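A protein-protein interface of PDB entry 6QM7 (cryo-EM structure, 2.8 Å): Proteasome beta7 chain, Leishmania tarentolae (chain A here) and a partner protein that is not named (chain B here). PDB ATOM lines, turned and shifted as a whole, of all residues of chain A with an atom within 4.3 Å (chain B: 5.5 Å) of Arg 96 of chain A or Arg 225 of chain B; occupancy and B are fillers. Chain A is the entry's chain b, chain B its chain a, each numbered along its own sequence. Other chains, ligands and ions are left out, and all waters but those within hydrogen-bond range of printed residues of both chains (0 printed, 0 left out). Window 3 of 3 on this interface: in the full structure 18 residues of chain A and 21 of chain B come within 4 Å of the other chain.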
ATOM      1  N   ILE A  92     -13.013 -36.283 -15.050  1.00  0.00           N
ATOM      2  CA  ILE A  92     -13.851 -35.058 -14.962  1.00  0.00           C
ATOM      3  C   ILE A  92     -13.328 -34.033 -15.957  1.00  0.00           C
ATOM      4  O   ILE A  92     -14.158 -33.351 -16.562  1.00  0.00           O
ATOM      5  CB  ILE A  92     -13.874 -34.513 -13.526  1.00  0.00           C
ATOM      6  CG1 ILE A  92     -14.747 -35.399 -12.641  1.00  0.00           C
ATOM      7  CG2 ILE A  92     -14.335 -33.061 -13.470  1.00  0.00           C
ATOM      8  CD1 ILE A  92     -14.550 -35.169 -11.160  1.00  0.00           C
ATOM      9  N   TYR A  93     -12.011 -33.895 -16.067  1.00  0.00           N
ATOM     10  CA  TYR A  93     -11.360 -32.937 -16.994  1.00  0.00           C
ATOM     11  C   TYR A  93     -11.609 -33.366 -18.435  1.00  0.00           C
ATOM     12  O   TYR A  93     -11.781 -32.481 -19.262  1.00  0.00           O
ATOM     13  CB  TYR A  93      -9.850 -32.838 -16.779  1.00  0.00           C
ATOM     14  CG  TYR A  93      -9.169 -31.890 -17.729  1.00  0.00           C
ATOM     15  CD1 TYR A  93      -9.251 -30.516 -17.557  1.00  0.00           C
ATOM     16  CD2 TYR A  93      -8.479 -32.360 -18.830  1.00  0.00           C
ATOM     17  CE1 TYR A  93      -8.666 -29.635 -18.452  1.00  0.00           C
ATOM     18  CE2 TYR A  93      -7.855 -31.496 -19.717  1.00  0.00           C
ATOM     19  CZ  TYR A  93      -7.946 -30.130 -19.528  1.00  0.00           C
ATOM     20  OH  TYR A  93      -7.343 -29.291 -20.427  1.00  0.00           O
ATOM     21  N   GLN A  94     -11.609 -34.661 -18.735  1.00  0.00           N
ATOM     22  CA  GLN A  94     -11.880 -35.137 -20.111  1.00  0.00           C
ATOM     23  C   GLN A  94     -13.298 -34.721 -20.474  1.00  0.00           C
ATOM     24  O   GLN A  94     -13.507 -34.300 -21.608  1.00  0.00           O
ATOM     25  CB  GLN A  94     -11.701 -36.653 -20.254  1.00  0.00           C
ATOM     26  CG  GLN A  94     -11.827 -37.153 -21.698  1.00  0.00           C
ATOM     27  CD  GLN A  94     -11.006 -36.337 -22.679  1.00  0.00           C
ATOM     28  OE1 GLN A  94      -9.805 -36.118 -22.493  1.00  0.00           O
ATOM     29  NE2 GLN A  94     -11.650 -35.853 -23.731  1.00  0.00           N
ATOM     30  N   LYS A  95     -14.225 -34.827 -19.525  1.00  0.00           N
ATOM     31  CA  LYS A  95     -15.649 -34.492 -19.740  1.00  0.00           C
ATOM     32  C   LYS A  95     -15.788 -32.995 -19.996  1.00  0.00           C
ATOM     33  O   LYS A  95     -16.687 -32.646 -20.740  1.00  0.00           O
ATOM     34  CB  LYS A  95     -16.508 -34.915 -18.548  1.00  0.00           C
ATOM     35  CG  LYS A  95     -16.581 -36.413 -18.294  1.00  0.00           C
ATOM     36  CD  LYS A  95     -17.910 -36.869 -17.729  1.00  0.00           C
ATOM     37  CE  LYS A  95     -18.973 -37.042 -18.792  1.00  0.00           C
ATOM     38  NZ  LYS A  95     -20.314 -36.678 -18.271  1.00  0.00           N
ATOM     39  N   ARG A  96     -14.959 -32.134 -19.415  1.00  0.00           N
ATOM     40  CA  ARG A  96     -15.097 -30.670 -19.639  1.00  0.00           C
ATOM     41  C   ARG A  96     -14.474 -30.313 -20.983  1.00  0.00           C
ATOM     42  O   ARG A  96     -14.882 -29.284 -21.557  1.00  0.00           O
ATOM     43  CB  ARG A  96     -14.535 -29.847 -18.476  1.00  0.00           C
ATOM     44  CG  ARG A  96     -13.089 -29.412 -18.595  1.00  0.00           C
ATOM     45  CD  ARG A  96     -12.890 -27.992 -19.088  1.00  0.00           C
ATOM     46  NE  ARG A  96     -11.631 -27.955 -19.817  1.00  0.00           N
ATOM     47  CZ  ARG A  96     -10.987 -26.867 -20.196  1.00  0.00           C
ATOM     48  NH1 ARG A  96      -9.860 -26.979 -20.880  1.00  0.00           N
ATOM     49  NH2 ARG A  96     -11.468 -25.672 -19.923  1.00  0.00           N
ATOM     50  N   CYS A  97     -13.539 -31.131 -21.457  1.00  0.00           N
ATOM     51  CA  CYS A  97     -12.890 -30.980 -22.777  1.00  0.00           C
ATOM     52  C   CYS A  97     -13.832 -31.450 -23.888  1.00  0.00           C
ATOM     53  O   CYS A  97     -13.674 -30.952 -25.017  1.00  0.00           O
ATOM     54  CB  CYS A  97     -11.560 -31.719 -22.809  1.00  0.00           C
ATOM     55  SG  CYS A  97     -10.365 -31.014 -21.644  1.00  0.00           S
ATOM     56  N   ASP A  98     -14.785 -32.334 -23.585  1.00  0.00           N
ATOM     57  CA  ASP A  98     -15.837 -32.789 -24.534  1.00  0.00           C
ATOM     58  C   ASP A  98     -17.058 -31.861 -24.479  1.00  0.00           C
ATOM     59  O   ASP A  98     -18.014 -32.135 -25.225  1.00  0.00           O
ATOM     60  CB  ASP A  98     -16.247 -34.237 -24.251  1.00  0.00           C
ATOM     61  CG  ASP A  98     -15.092 -35.227 -24.284  1.00  0.00           C
ATOM     62  OD1 ASP A  98     -15.291 -36.380 -23.845  1.00  0.00           O
ATOM     63  OD2 ASP A  98     -13.996 -34.836 -24.741  1.00  0.00           O
ATOM     64  N   PHE A  99     -17.040 -30.822 -23.629  1.00  0.00           N
ATOM     65  CA  PHE A  99     -18.170 -29.887 -23.366  1.00  0.00           C
ATOM     66  C   PHE A  99     -19.403 -30.665 -22.890  1.00  0.00           C
ATOM     67  O   PHE A  99     -20.531 -30.167 -23.080  1.00  0.00           O
ATOM     68  CB  PHE A  99     -18.462 -29.043 -24.608  1.00  0.00           C
ATOM     69  CG  PHE A  99     -17.447 -27.961 -24.861  1.00  0.00           C
ATOM     70  CD1 PHE A  99     -17.684 -26.659 -24.437  1.00  0.00           C
ATOM     71  CD2 PHE A  99     -16.250 -28.247 -25.505  1.00  0.00           C
ATOM     72  CE1 PHE A  99     -16.747 -25.662 -24.661  1.00  0.00           C
ATOM     73  CE2 PHE A  99     -15.311 -27.248 -25.721  1.00  0.00           C
ATOM     74  CZ  PHE A  99     -15.562 -25.958 -25.303  1.00  0.00           C
ATOM     75  N   ASP A 123     -16.047 -29.242 -11.500  1.00  0.00           N
ATOM     76  CA  ASP A 123     -16.614 -29.473 -12.855  1.00  0.00           C
ATOM     77  C   ASP A 123     -15.544 -29.377 -13.952  1.00  0.00           C
ATOM     78  O   ASP A 123     -15.601 -30.210 -14.890  1.00  0.00           O
ATOM     79  CB  ASP A 123     -17.752 -28.482 -13.144  1.00  0.00           C
ATOM     80  CG  ASP A 123     -17.577 -27.089 -12.532  1.00  0.00           C
ATOM     81  OD1 ASP A 123     -17.418 -26.114 -13.306  1.00  0.00           O
ATOM     82  OD2 ASP A 123     -17.619 -26.982 -11.265  1.00  0.00           O
ATOM     83  N   VAL A 124     -14.649 -28.384 -13.880  1.00  0.00           N
ATOM     84  CA  VAL A 124     -13.675 -28.042 -14.962  1.00  0.00           C
ATOM     85  C   VAL A 124     -12.345 -28.773 -14.774  1.00  0.00           C
ATOM     86  O   VAL A 124     -11.468 -28.589 -15.628  1.00  0.00           O
ATOM     87  CB  VAL A 124     -13.425 -26.528 -15.061  1.00  0.00           C
ATOM     88  CG1 VAL A 124     -14.676 -25.788 -15.491  1.00  0.00           C
ATOM     89  CG2 VAL A 124     -12.865 -25.939 -13.772  1.00  0.00           C
ATOM     90  N   TRP B 126     -22.488 -22.342 -17.825  1.00  0.00           N
ATOM     91  CA  TRP B 126     -21.254 -23.105 -17.479  1.00  0.00           C
ATOM     92  C   TRP B 126     -20.140 -22.757 -18.466  1.00  0.00           C
ATOM     93  O   TRP B 126     -20.277 -23.111 -19.653  1.00  0.00           O
ATOM     94  CB  TRP B 126     -21.502 -24.614 -17.484  1.00  0.00           C
ATOM     95  CG  TRP B 126     -20.264 -25.397 -17.176  1.00  0.00           C
ATOM     96  CD1 TRP B 126     -19.747 -25.646 -15.939  1.00  0.00           C
ATOM     97  CD2 TRP B 126     -19.360 -26.006 -18.116  1.00  0.00           C
ATOM     98  NE1 TRP B 126     -18.601 -26.386 -16.043  1.00  0.00           N
ATOM     99  CE2 TRP B 126     -18.339 -26.622 -17.361  1.00  0.00           C
ATOM    100  CE3 TRP B 126     -19.315 -26.101 -19.514  1.00  0.00           C
ATOM    101  CZ2 TRP B 126     -17.282 -27.309 -17.954  1.00  0.00           C
ATOM    102  CZ3 TRP B 126     -18.279 -26.796 -20.102  1.00  0.00           C
ATOM    103  CH2 TRP B 126     -17.280 -27.395 -19.330  1.00  0.00           C
ATOM    104  N   PRO B 128     -16.246 -23.535 -19.578  1.00  0.00           N
ATOM    105  CA  PRO B 128     -15.175 -24.515 -19.417  1.00  0.00           C
ATOM    106  C   PRO B 128     -13.907 -23.902 -18.804  1.00  0.00           C
ATOM    107  O   PRO B 128     -13.042 -24.660 -18.413  1.00  0.00           O
ATOM    108  CB  PRO B 128     -14.888 -24.980 -20.853  1.00  0.00           C
ATOM    109  CG  PRO B 128     -15.250 -23.782 -21.690  1.00  0.00           C
ATOM    110  CD  PRO B 128     -16.444 -23.164 -20.989  1.00  0.00           C
ATOM    111  N   TYR B 129     -13.832 -22.570 -18.741  1.00  0.00           N
ATOM    112  CA  TYR B 129     -12.686 -21.794 -18.215  1.00  0.00           C
ATOM    113  C   TYR B 129     -13.008 -21.239 -16.828  1.00  0.00           C
ATOM    114  O   TYR B 129     -14.173 -20.921 -16.544  1.00  0.00           O
ATOM    115  CB  TYR B 129     -12.358 -20.653 -19.172  1.00  0.00           C
ATOM    116  CG  TYR B 129     -11.899 -21.091 -20.540  1.00  0.00           C
ATOM    117  CD1 TYR B 129     -12.531 -20.628 -21.686  1.00  0.00           C
ATOM    118  CD2 TYR B 129     -10.813 -21.944 -20.699  1.00  0.00           C
ATOM    119  CE1 TYR B 129     -12.098 -21.000 -22.949  1.00  0.00           C
ATOM    120  CE2 TYR B 129     -10.353 -22.311 -21.955  1.00  0.00           C
ATOM    121  CZ  TYR B 129     -10.997 -21.834 -23.088  1.00  0.00           C
ATOM    122  OH  TYR B 129     -10.576 -22.179 -24.340  1.00  0.00           O
ATOM    123  N   MET B 182      -5.836 -20.846 -15.644  1.00  0.00           N
ATOM    124  CA  MET B 182      -6.691 -21.949 -15.170  1.00  0.00           C
ATOM    125  C   MET B 182      -5.802 -23.095 -14.724  1.00  0.00           C
ATOM    126  O   MET B 182      -4.929 -23.472 -15.502  1.00  0.00           O
ATOM    127  CB  MET B 182      -7.591 -22.455 -16.295  1.00  0.00           C
ATOM    128  CG  MET B 182      -8.405 -23.622 -15.869  1.00  0.00           C
ATOM    129  SD  MET B 182     -10.047 -23.599 -16.532  1.00  0.00           S
ATOM    130  CE  MET B 182     -10.050 -25.186 -17.360  1.00  0.00           C
ATOM    131  N   ASP B 185      -6.061 -26.657 -16.733  1.00  0.00           N
ATOM    132  CA  ASP B 185      -5.377 -26.613 -18.048  1.00  0.00           C
ATOM    133  C   ASP B 185      -3.871 -26.662 -17.841  1.00  0.00           C
ATOM    134  O   ASP B 185      -3.190 -27.361 -18.585  1.00  0.00           O
ATOM    135  CB  ASP B 185      -5.789 -25.373 -18.836  1.00  0.00           C
ATOM    136  CG  ASP B 185      -7.084 -25.584 -19.599  1.00  0.00           C
ATOM    137  OD1 ASP B 185      -7.652 -26.686 -19.483  1.00  0.00           O
ATOM    138  OD2 ASP B 185      -7.503 -24.653 -20.323  1.00  0.00           O
ATOM    139  N   GLN B 188      -3.148 -30.190 -17.327  1.00  0.00           N
ATOM    140  CA  GLN B 188      -3.219 -30.987 -18.574  1.00  0.00           C
ATOM    141  C   GLN B 188      -1.965 -30.701 -19.396  1.00  0.00           C
ATOM    142  O   GLN B 188      -1.261 -31.658 -19.760  1.00  0.00           O
ATOM    143  CB  GLN B 188      -4.464 -30.667 -19.400  1.00  0.00           C
ATOM    144  CG  GLN B 188      -4.573 -31.502 -20.669  1.00  0.00           C
ATOM    145  CD  GLN B 188      -4.785 -32.981 -20.426  1.00  0.00           C
ATOM    146  OE1 GLN B 188      -4.711 -33.786 -21.351  1.00  0.00           O
ATOM    147  NE2 GLN B 188      -5.070 -33.356 -19.186  1.00  0.00           N
ATOM    148  N   THR B 220       4.323 -24.541 -30.049  1.00  0.00           N
ATOM    149  CA  THR B 220       3.697 -25.411 -31.064  1.00  0.00           C
ATOM    150  C   THR B 220       2.460 -26.056 -30.452  1.00  0.00           C
ATOM    151  O   THR B 220       1.430 -26.059 -31.114  1.00  0.00           O
ATOM    152  CB  THR B 220       4.721 -26.440 -31.553  1.00  0.00           C
ATOM    153  OG1 THR B 220       5.796 -25.749 -32.193  1.00  0.00           O
ATOM    154  CG2 THR B 220       4.115 -27.437 -32.510  1.00  0.00           C
ATOM    155  N   MET B 221       2.561 -26.562 -29.229  1.00  0.00           N
ATOM    156  CA  MET B 221       1.461 -27.285 -28.542  1.00  0.00           C
ATOM    157  C   MET B 221       0.363 -26.318 -28.126  1.00  0.00           C
ATOM    158  O   MET B 221      -0.807 -26.730 -28.163  1.00  0.00           O
ATOM    159  CB  MET B 221       1.962 -27.995 -27.288  1.00  0.00           C
ATOM    160  CG  MET B 221       2.908 -29.126 -27.598  1.00  0.00           C
ATOM    161  SD  MET B 221       3.353 -29.919 -26.068  1.00  0.00           S
ATOM    162  CE  MET B 221       1.813 -30.783 -25.759  1.00  0.00           C
ATOM    163  N   LEU B 222       0.726 -25.107 -27.711  1.00  0.00           N
ATOM    164  CA  LEU B 222      -0.252 -24.027 -27.417  1.00  0.00           C
ATOM    165  C   LEU B 222      -0.985 -23.641 -28.688  1.00  0.00           C
ATOM    166  O   LEU B 222      -2.183 -23.393 -28.581  1.00  0.00           O
ATOM    167  CB  LEU B 222       0.445 -22.794 -26.843  1.00  0.00           C
ATOM    168  CG  LEU B 222       0.491 -22.637 -25.320  1.00  0.00           C
ATOM    169  CD1 LEU B 222       0.314 -23.952 -24.561  1.00  0.00           C
ATOM    170  CD2 LEU B 222       1.801 -21.963 -24.912  1.00  0.00           C
ATOM    171  N   TYR B 223      -0.296 -23.558 -29.825  1.00  0.00           N
ATOM    172  CA  TYR B 223      -0.907 -23.132 -31.112  1.00  0.00           C
ATOM    173  C   TYR B 223      -1.805 -24.243 -31.653  1.00  0.00           C
ATOM    174  O   TYR B 223      -2.837 -23.925 -32.231  1.00  0.00           O
ATOM    175  CB  TYR B 223       0.117 -22.733 -32.182  1.00  0.00           C
ATOM    176  CG  TYR B 223      -0.532 -21.912 -33.268  1.00  0.00           C
ATOM    177  CD1 TYR B 223      -0.888 -20.597 -33.022  1.00  0.00           C
ATOM    178  CD2 TYR B 223      -0.910 -22.468 -34.479  1.00  0.00           C
ATOM    179  CE1 TYR B 223      -1.527 -19.825 -33.971  1.00  0.00           C
ATOM    180  CE2 TYR B 223      -1.561 -21.714 -35.444  1.00  0.00           C
ATOM    181  CZ  TYR B 223      -1.869 -20.388 -35.184  1.00  0.00           C
ATOM    182  OH  TYR B 223      -2.511 -19.615 -36.106  1.00  0.00           O
ATOM    183  N   HIS B 224      -1.433 -25.503 -31.458  1.00  0.00           N
ATOM    184  CA  HIS B 224      -2.231 -26.644 -31.960  1.00  0.00           C
ATOM    185  C   HIS B 224      -3.582 -26.678 -31.263  1.00  0.00           C
ATOM    186  O   HIS B 224      -4.460 -27.388 -31.767  1.00  0.00           O
ATOM    187  CB  HIS B 224      -1.478 -27.971 -31.824  1.00  0.00           C
ATOM    188  CG  HIS B 224      -0.418 -28.169 -32.857  1.00  0.00           C
ATOM    189  ND1 HIS B 224       0.495 -29.206 -32.780  1.00  0.00           N
ATOM    190  CD2 HIS B 224      -0.101 -27.461 -33.970  1.00  0.00           C
ATOM    191  CE1 HIS B 224       1.311 -29.140 -33.816  1.00  0.00           C
ATOM    192  NE2 HIS B 224       0.972 -28.075 -34.558  1.00  0.00           N
ATOM    193  N   ARG B 225      -3.742 -25.945 -30.165  1.00  0.00           N
ATOM    194  CA  ARG B 225      -5.015 -25.872 -29.413  1.00  0.00           C
ATOM    195  C   ARG B 225      -5.662 -24.508 -29.622  1.00  0.00           C
ATOM    196  O   ARG B 225      -6.573 -24.224 -28.868  1.00  0.00           O
ATOM    197  CB  ARG B 225      -4.769 -26.182 -27.931  1.00  0.00           C
ATOM    198  CG  ARG B 225      -4.867 -27.662 -27.568  1.00  0.00           C
ATOM    199  CD  ARG B 225      -6.295 -28.163 -27.421  1.00  0.00           C
ATOM    200  NE  ARG B 225      -6.954 -27.530 -26.284  1.00  0.00           N
ATOM    201  CZ  ARG B 225      -7.046 -28.027 -25.049  1.00  0.00           C
ATOM    202  NH1 ARG B 225      -6.537 -29.212 -24.747  1.00  0.00           N
ATOM    203  NH2 ARG B 225      -7.657 -27.328 -24.102  1.00  0.00           N
ATOM    204  N   ARG B 226      -5.324 -23.743 -30.660  1.00  0.00           N
ATOM    205  CA  ARG B 226      -5.775 -22.326 -30.752  1.00  0.00           C
ATOM    206  C   ARG B 226      -7.271 -22.187 -31.076  1.00  0.00           C
ATOM    207  O   ARG B 226      -7.723 -21.030 -31.122  1.00  0.00           O
ATOM    208  CB  ARG B 226      -4.923 -21.501 -31.721  1.00  0.00           C
ATOM    209  CG  ARG B 226      -5.083 -21.781 -33.208  1.00  0.00           C
ATOM    210  CD  ARG B 226      -5.410 -20.541 -34.034  1.00  0.00           C
ATOM    211  NE  ARG B 226      -5.137 -19.223 -33.426  1.00  0.00           N
ATOM    212  CZ  ARG B 226      -5.939 -18.139 -33.460  1.00  0.00           C
ATOM    213  NH1 ARG B 226      -7.123 -18.153 -34.059  1.00  0.00           N
ATOM    214  NH2 ARG B 226      -5.541 -17.023 -32.873  1.00  0.00           N
ATOM    215  N   PHE B 227      -8.021 -23.281 -31.261  1.00  0.00           N
ATOM    216  CA  PHE B 227      -9.484 -23.264 -31.541  1.00  0.00           C
ATOM    217  C   PHE B 227     -10.286 -23.711 -30.308  1.00  0.00           C
ATOM    218  O   PHE B 227     -11.526 -23.574 -30.341  1.00  0.00           O
ATOM    219  CB  PHE B 227      -9.773 -24.083 -32.803  1.00  0.00           C
ATOM    220  CG  PHE B 227      -9.020 -23.586 -34.017  1.00  0.00           C
ATOM    221  CD1 PHE B 227      -9.139 -22.264 -34.442  1.00  0.00           C
ATOM    222  CD2 PHE B 227      -8.165 -24.427 -34.721  1.00  0.00           C
ATOM    223  CE1 PHE B 227      -8.431 -21.805 -35.545  1.00  0.00           C
ATOM    224  CE2 PHE B 227      -7.457 -23.964 -35.826  1.00  0.00           C
ATOM    225  CZ  PHE B 227      -7.585 -22.652 -36.234  1.00  0.00           C
ATOM    226  N   PHE B 228      -9.616 -24.224 -29.267  1.00  0.00           N
ATOM    227  CA  PHE B 228     -10.111 -24.306 -27.862  1.00  0.00           C
ATOM    228  C   PHE B 228      -8.908 -24.167 -26.925  1.00  0.00           C
ATOM    229  O   PHE B 228      -8.469 -25.135 -26.306  1.00  0.00           O
ATOM    230  CB  PHE B 228     -10.910 -25.595 -27.633  1.00  0.00           C
ATOM    231  CG  PHE B 228     -11.331 -25.835 -26.203  1.00  0.00           C
ATOM    232  CD1 PHE B 228     -11.912 -24.820 -25.451  1.00  0.00           C
ATOM    233  CD2 PHE B 228     -11.141 -27.074 -25.602  1.00  0.00           C
ATOM    234  CE1 PHE B 228     -12.287 -25.038 -24.131  1.00  0.00           C
ATOM    235  CE2 PHE B 228     -11.521 -27.292 -24.283  1.00  0.00           C
ATOM    236  CZ  PHE B 228     -12.091 -26.272 -23.549  1.00  0.00           C
ATOM    237  N   PRO B 229      -8.304 -22.961 -26.832  1.00  0.00           N
ATOM    238  CA  PRO B 229      -6.989 -22.803 -26.210  1.00  0.00           C
ATOM    239  C   PRO B 229      -6.943 -23.205 -24.731  1.00  0.00           C
ATOM    240  O   PRO B 229      -7.958 -23.130 -24.069  1.00  0.00           O
ATOM    241  CB  PRO B 229      -6.629 -21.319 -26.399  1.00  0.00           C
ATOM    242  CG  PRO B 229      -7.922 -20.631 -26.789  1.00  0.00           C
ATOM    243  CD  PRO B 229      -8.836 -21.698 -27.357  1.00  0.00           C
ATOM    244  N   TYR B 230      -5.775 -23.666 -24.276  1.00  0.00           N
ATOM    245  CA  TYR B 230      -5.461 -23.813 -22.837  1.00  0.00           C
ATOM    246  C   TYR B 230      -5.473 -22.413 -22.231  1.00  0.00           C
ATOM    247  O   TYR B 230      -4.736 -21.558 -22.736  1.00  0.00           O
ATOM    248  CB  TYR B 230      -4.077 -24.402 -22.590  1.00  0.00           C
ATOM    249  CG  TYR B 230      -3.817 -25.807 -23.064  1.00  0.00           C
ATOM    250  CD1 TYR B 230      -4.267 -26.905 -22.349  1.00  0.00           C
ATOM    251  CD2 TYR B 230      -3.019 -26.048 -24.173  1.00  0.00           C
ATOM    252  CE1 TYR B 230      -3.984 -28.202 -22.757  1.00  0.00           C
ATOM    253  CE2 TYR B 230      -2.723 -27.336 -24.587  1.00  0.00           C
ATOM    254  CZ  TYR B 230      -3.206 -28.417 -23.879  1.00  0.00           C
ATOM    255  OH  TYR B 230      -2.913 -29.680 -24.299  1.00  0.00           O
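OD1 of Asp 185 of chain B is in hydrogen-bond range of OH of Tyr 93 of chain A, at 2.8 Å.
The guanidinium group (NH2) of Arg 96 of chain A sits at hydrogen-bond distance from the backbone carbonyl oxygen (O) of Pro 128 of chain B, 2.4 Å away.
The side-chain carboxylate of Asp 123 of chain A is in hydrogen-bond range of the indole nitrogen of Trp 126 of chain B (3.0 Å).
OD1 of Asp 185 of chain B lies within salt-bridge range of NH1 of Arg 96 of chain A (2.6 Å).
Tyr 93 of chain A touches Gln 188 of chain B (OH to CB, 3.4 Å).
CZ2 of Trp 126 of chain B touches CB of Arg 96 of chain A, at 3.8 Å.
Tyr 129 of chain B touches Arg 96 of chain A.
Met 182 of chain B touches Arg 96 of chain A (CE to NH2, 3.0 Å).
Arg 96 of chain A touches Arg 225 of chain B (NH1 to NH2, 3.9 Å).
Arg 96 of chain A touches Phe 228 of chain B.
CG of Pro 128 of chain B touches CE1 of Phe 99 of chain A (3.8 Å).
CE1 of Phe 228 of chain B touches CZ of Phe 99 of chain A, 3.6 Å away.
CZ2 of Trp 126 of chain B touches CG1 of Val 124 of chain A, at 3.9 Å.
Pro 128 of chain B touches Val 124 of chain A.
OH of Tyr 129 of chain B sits at hydrogen-bond distance from O of Pro 229 of chain B.
The backbone carbonyl oxygen (O) of Tyr 93 of chain A is in hydrogen-bond range of the side-chain sulfur (SG) of Cys 97 of chain A.
The backbone carbonyl oxygen of Phe 228 of chain B is in hydrogen-bond range of the guanidinium group of Arg 225 of chain B (2.8 Å).
The side-chain hydroxyl of Tyr 93 of chain A is in hydrogen-bond range of the guanidinium group of Arg 96 of chain A, 3.4 Å away.
The guanidinium group of Arg 96 of chain A lies within hydrogen-bond range of the side-chain sulfur of Cys 97 of chain A, at 3.8 Å.
Printed residues of chain B that touch a printed residue of chain A: Trp 126, Pro 128, Tyr 129, Met 182, Asp 185, Gln 188, Arg 225 and Phe 228.
Hydrophobic or aromatic side chains of chain B that line the printed part of chain A: Trp 126, Pro 128, Tyr 129, Met 182 and Phe 228.
Of the 10 printed residues of chain A, 5 touch a printed residue of chain B.
Of the printed residues of chain B, Tyr 93 of chain A touches Asp 185 (2.8 Å) and Gln 188 (3.4 Å).
Arg 96 of chain A touches seven residues of chain B.
Printed residues of chain B within 4 Å of Asp 123 of chain A: Trp 126 (3.0 Å).
Printed residues of chain A within 4 Å of Pro 128 of chain B: Arg 96, Phe 99 and Val 124.
Printed residues of chain A within 4 Å of Tyr 129 of chain B: Arg 96.
Printed residues of chain A within 4 Å of Asp 185 of chain B: Tyr 93 and Arg 96.
The nearest residue of chain B that does not touch Arg 96 of chain A is Pro 229 of chain B (5.3 Å).
The nearest printed residue of chain A that does not touch Trp 126 of chain B is Phe 99 of chain A (4.4 Å).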
